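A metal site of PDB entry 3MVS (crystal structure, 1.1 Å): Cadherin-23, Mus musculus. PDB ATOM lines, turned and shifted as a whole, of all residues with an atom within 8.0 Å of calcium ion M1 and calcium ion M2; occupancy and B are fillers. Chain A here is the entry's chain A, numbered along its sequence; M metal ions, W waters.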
ATOM      1  N   GLU A 120      19.982   2.738   3.701  1.00  0.00           N
ATOM      2  CA  GLU A 120      20.087   3.349   2.374  1.00  0.00           C
ATOM      3  C   GLU A 120      20.991   2.549   1.432  1.00  0.00           C
ATOM      4  O   GLU A 120      20.880   2.719   0.217  1.00  0.00           O
ATOM      5  CB  GLU A 120      20.535   4.817   2.397  1.00  0.00           C
ATOM      6  CG  GLU A 120      21.941   5.029   2.966  1.00  0.00           C
ATOM      7  CD  GLU A 120      22.422   6.456   2.802  1.00  0.00           C
ATOM      8  OE1 GLU A 120      22.186   7.064   1.727  1.00  0.00           O
ATOM      9  OE2 GLU A 120      23.070   6.956   3.749  1.00  0.00           O
ATOM     10  N   ASN A 121      21.861   1.676   1.967  1.00  0.00           N
ATOM     11  CA  ASN A 121      22.694   0.832   1.099  1.00  0.00           C
ATOM     12  C   ASN A 121      22.135  -0.586   0.894  1.00  0.00           C
ATOM     13  O   ASN A 121      22.853  -1.486   0.479  1.00  0.00           O
ATOM     14  CB  ASN A 121      24.151   0.795   1.567  1.00  0.00           C
ATOM     15  CG  ASN A 121      24.317   0.105   2.909  1.00  0.00           C
ATOM     16  OD1 ASN A 121      23.351  -0.145   3.620  1.00  0.00           O
ATOM     17  ND2 ASN A 121      25.563  -0.212   3.238  1.00  0.00           N
ATOM     18  N   GLU A 169      18.766   2.058  -6.358  1.00  0.00           N
ATOM     19  CA  GLU A 169      19.570   2.445  -5.225  1.00  0.00           C
ATOM     20  C   GLU A 169      18.917   3.580  -4.428  1.00  0.00           C
ATOM     21  O   GLU A 169      18.442   4.582  -4.991  1.00  0.00           O
ATOM     22  CB  GLU A 169      20.947   2.891  -5.689  1.00  0.00           C
ATOM     23  CG  GLU A 169      21.823   3.335  -4.532  1.00  0.00           C
ATOM     24  CD  GLU A 169      23.270   3.519  -4.881  1.00  0.00           C
ATOM     25  OE1 GLU A 169      23.590   3.621  -6.081  1.00  0.00           O
ATOM     26  OE2 GLU A 169      24.094   3.565  -3.933  1.00  0.00           O
ATOM     27  N   LEU A 170      18.924   3.420  -3.097  1.00  0.00           N
ATOM     28  CA  LEU A 170      18.338   4.410  -2.191  1.00  0.00           C
ATOM     29  C   LEU A 170      19.383   5.433  -1.771  1.00  0.00           C
ATOM     30  O   LEU A 170      20.567   5.213  -1.966  1.00  0.00           O
ATOM     31  CB  LEU A 170      17.749   3.690  -0.976  1.00  0.00           C
ATOM     32  CG  LEU A 170      16.706   2.627  -1.320  1.00  0.00           C
ATOM     33  CD1 LEU A 170      16.560   1.556  -0.218  1.00  0.00           C
ATOM     34  CD2 LEU A 170      15.365   3.293  -1.643  1.00  0.00           C
ATOM     35  N   ASP A 171      18.936   6.553  -1.247  1.00  0.00           N
ATOM     36  CA  ASP A 171      19.842   7.611  -0.834  1.00  0.00           C
ATOM     37  C   ASP A 171      19.171   8.454   0.243  1.00  0.00           C
ATOM     38  O   ASP A 171      18.297   9.281  -0.068  1.00  0.00           O
ATOM     39  CB  ASP A 171      20.252   8.478  -2.043  1.00  0.00           C
ATOM     40  CG  ASP A 171      21.335   9.470  -1.693  1.00  0.00           C
ATOM     41  OD1 ASP A 171      21.795   9.505  -0.530  1.00  0.00           O
ATOM     42  OD2 ASP A 171      21.735  10.218  -2.617  1.00  0.00           O
ATOM     43  N   TYR A 172      19.575   8.252   1.498  1.00  0.00           N
ATOM     44  CA  TYR A 172      19.008   8.946   2.620  1.00  0.00           C
ATOM     45  C   TYR A 172      19.111  10.461   2.432  1.00  0.00           C
ATOM     46  O   TYR A 172      18.230  11.211   2.848  1.00  0.00           O
ATOM     47  CB  TYR A 172      19.769   8.530   3.899  1.00  0.00           C
ATOM     48  CG  TYR A 172      19.265   9.238   5.103  1.00  0.00           C
ATOM     49  CD1 TYR A 172      18.235   8.679   5.871  1.00  0.00           C
ATOM     50  CD2 TYR A 172      19.808  10.463   5.504  1.00  0.00           C
ATOM     51  CE1 TYR A 172      17.749   9.345   7.007  1.00  0.00           C
ATOM     52  CE2 TYR A 172      19.331  11.136   6.618  1.00  0.00           C
ATOM     53  CZ  TYR A 172      18.297  10.567   7.364  1.00  0.00           C
ATOM     54  OH  TYR A 172      17.811  11.194   8.481  1.00  0.00           O
ATOM     55  N   GLU A 173      20.200  10.909   1.814  1.00  0.00           N
ATOM     56  CA  GLU A 173      20.455  12.325   1.594  1.00  0.00           C
ATOM     57  C   GLU A 173      19.429  12.973   0.640  1.00  0.00           C
ATOM     58  O   GLU A 173      19.339  14.195   0.558  1.00  0.00           O
ATOM     59  CB  GLU A 173      21.888  12.518   1.081  1.00  0.00           C
ATOM     60  CG  GLU A 173      22.983  12.461   2.175  1.00  0.00           C
ATOM     61  CD  GLU A 173      23.261  11.077   2.785  1.00  0.00           C
ATOM     62  OE1 GLU A 173      23.167  10.024   2.127  1.00  0.00           O
ATOM     63  OE2 GLU A 173      23.607  11.051   3.987  1.00  0.00           O
ATOM     64  N   VAL A 174      18.694  12.146  -0.088  1.00  0.00           N
ATOM     65  CA  VAL A 174      17.604  12.628  -0.944  1.00  0.00           C
ATOM     66  C   VAL A 174      16.255  12.380  -0.264  1.00  0.00           C
ATOM     67  O   VAL A 174      15.445  13.289  -0.130  1.00  0.00           O
ATOM     68  CB  VAL A 174      17.644  11.962  -2.339  1.00  0.00           C
ATOM     69  CG1 VAL A 174      16.400  12.364  -3.148  1.00  0.00           C
ATOM     70  CG2 VAL A 174      18.911  12.366  -3.089  1.00  0.00           C
ATOM     71  N   ILE A 203      14.164   5.020   5.940  1.00  0.00           N
ATOM     72  CA  ILE A 203      15.531   4.815   5.455  1.00  0.00           C
ATOM     73  C   ILE A 203      16.520   5.154   6.568  1.00  0.00           C
ATOM     74  O   ILE A 203      16.480   6.251   7.124  1.00  0.00           O
ATOM     75  CB  ILE A 203      15.821   5.676   4.204  1.00  0.00           C
ATOM     76  CG1 ILE A 203      14.747   5.458   3.108  1.00  0.00           C
ATOM     77  CG2 ILE A 203      17.213   5.373   3.679  1.00  0.00           C
ATOM     78  CD1 ILE A 203      14.589   4.007   2.636  1.00  0.00           C
ATOM     79  N   THR A 204      17.393   4.199   6.895  1.00  0.00           N
ATOM     80  CA  THR A 204      18.523   4.421   7.806  1.00  0.00           C
ATOM     81  C   THR A 204      19.663   5.123   7.081  1.00  0.00           C
ATOM     82  O   THR A 204      20.105   4.686   6.006  1.00  0.00           O
ATOM     83  CB  THR A 204      18.974   3.089   8.337  1.00  0.00           C
ATOM     84  OG1 THR A 204      17.932   2.554   9.156  1.00  0.00           O
ATOM     85  CG2 THR A 204      20.255   3.187   9.202  1.00  0.00           C
ATOM     86  N   ASP A 205      20.104   6.239   7.635  1.00  0.00           N
ATOM     87  CA  ASP A 205      21.264   6.952   7.119  1.00  0.00           C
ATOM     88  C   ASP A 205      22.504   6.123   7.392  1.00  0.00           C
ATOM     89  O   ASP A 205      22.788   5.773   8.531  1.00  0.00           O
ATOM     90  CB  ASP A 205      21.349   8.298   7.831  1.00  0.00           C
ATOM     91  CG  ASP A 205      22.398   9.217   7.242  1.00  0.00           C
ATOM     92  OD1 ASP A 205      22.887   8.923   6.132  1.00  0.00           O
ATOM     93  OD2 ASP A 205      22.710  10.221   7.924  1.00  0.00           O
ATOM     94  N   MET A 206      23.244   5.780   6.350  1.00  0.00           N
ATOM     95  CA  MET A 206      24.518   5.102   6.487  1.00  0.00           C
ATOM     96  C   MET A 206      25.651   6.098   6.305  1.00  0.00           C
ATOM     97  O   MET A 206      25.476   7.139   5.667  1.00  0.00           O
ATOM     98  CB  MET A 206      24.632   3.966   5.469  1.00  0.00           C
ATOM     99  CG  MET A 206      23.527   2.932   5.572  1.00  0.00           C
ATOM    100  SD  MET A 206      23.415   2.071   7.155  1.00  0.00           S
ATOM    101  CE  MET A 206      24.877   1.069   7.022  1.00  0.00           C
ATOM    102  N   GLN A 207      26.804   5.795   6.885  1.00  0.00           N
ATOM    103  CA  GLN A 207      27.956   6.673   6.777  1.00  0.00           C
ATOM    104  C   GLN A 207      28.593   6.411   5.421  1.00  0.00           C
ATOM    105  O   GLN A 207      29.457   5.562   5.296  1.00  0.00           O
ATOM    106  CB  GLN A 207      28.904   6.440   7.959  1.00  0.00           C
ATOM    107  CG  GLN A 207      28.233   6.820   9.266  1.00  0.00           C
ATOM    108  CD  GLN A 207      29.225   6.912  10.378  1.00  0.00           C
ATOM    109  OE1 GLN A 207      30.117   7.770  10.338  1.00  0.00           O
ATOM    110  NE2 GLN A 207      29.094   6.047  11.383  1.00  0.00           N
ATOM    111  N   ASP A 208      28.117   7.113   4.401  1.00  0.00           N
ATOM    112  CA  ASP A 208      28.451   6.776   3.028  1.00  0.00           C
ATOM    113  C   ASP A 208      28.998   7.935   2.226  1.00  0.00           C
ATOM    114  O   ASP A 208      28.801   8.019   1.006  1.00  0.00           O
ATOM    115  CB  ASP A 208      27.221   6.159   2.312  1.00  0.00           C
ATOM    116  CG  ASP A 208      26.083   7.151   2.089  1.00  0.00           C
ATOM    117  OD1 ASP A 208      25.966   8.184   2.800  1.00  0.00           O
ATOM    118  OD2 ASP A 208      25.281   6.881   1.171  1.00  0.00           O
ATOM    119  N   MET A 209      29.693   8.859   2.902  1.00  0.00           N
ATOM    120  CA  MET A 209      30.295   9.974   2.181  1.00  0.00           C
ATOM    121  C   MET A 209      31.332   9.427   1.194  1.00  0.00           C
ATOM    122  O   MET A 209      32.127   8.562   1.550  1.00  0.00           O
ATOM    123  CB  MET A 209      30.923  10.968   3.155  1.00  0.00           C
ATOM    124  CG  MET A 209      31.083  12.368   2.576  1.00  0.00           C
ATOM    125  SD  MET A 209      31.512  13.618   3.798  1.00  0.00           S
ATOM    126  CE  MET A 209      30.263  13.372   5.055  1.00  0.00           C
ATOM    127  N   ASP A 210      31.277   9.886  -0.059  1.00  0.00           N
ATOM    128  CA  ASP A 210      32.279   9.523  -1.061  1.00  0.00           C
ATOM    129  C   ASP A 210      33.561  10.337  -0.858  1.00  0.00           C
ATOM    130  O   ASP A 210      33.527  11.404  -0.236  1.00  0.00           O
HETATM  131 CA    CA M   1      23.642   8.471   0.484  1.00  0.00          CA
HETATM  132 CA    CA M   2      24.388   8.842   4.417  1.00  0.00          CA
HETATM  133  O   HOH W   1      25.209  10.076  -0.206  1.00  0.00           O
HETATM  134  O   HOH W   2      23.236   6.862  -1.214  1.00  0.00           O
HETATM  135  O   HOH W   3      26.104   9.997   5.687  1.00  0.00           O
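Four residues have an atom within 4 Å of calcium ion M1: Glu 120, Asp 171, Glu 173 and Asp 208.
Calcium ion M1 is bound by OE1 of Glu 173 (2.3 Å). OD1 of Asp 171 is bound to calcium ion M1 (2.3 Å). Water W1 binds calcium ion M1, at 2.3 Å. Water W2 binds calcium ion M1 (2.4 Å). Calcium ion M1 is bound by the side-chain carboxylate (OE1) of Glu 120 (2.4 Å). OD2 of Asp 208 binds calcium ion M1 (2.4 Å).
N of Glu 120 lies within hydrogen-bond range of O of Thr 204, 3.0 Å away. OE1 of Glu 120 sits close to N of Tyr 172.
The nearest printed residue that does not touch calcium ion M2 is Gln 207 (4.6 Å).
Calcium ion M2 is bound by OD1 of Asp 205 (2.3 Å), OD1 of Asp 208 (2.4 Å), O of Met 206 (2.4 Å), OE2 of Glu 173 (2.4 Å), OE2 of Glu 120 (2.4 Å), water W3 (2.4 Å) and OE1 of Glu 173 (2.9 Å). Calcium ion M2 has seven donor atoms within binding distance.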
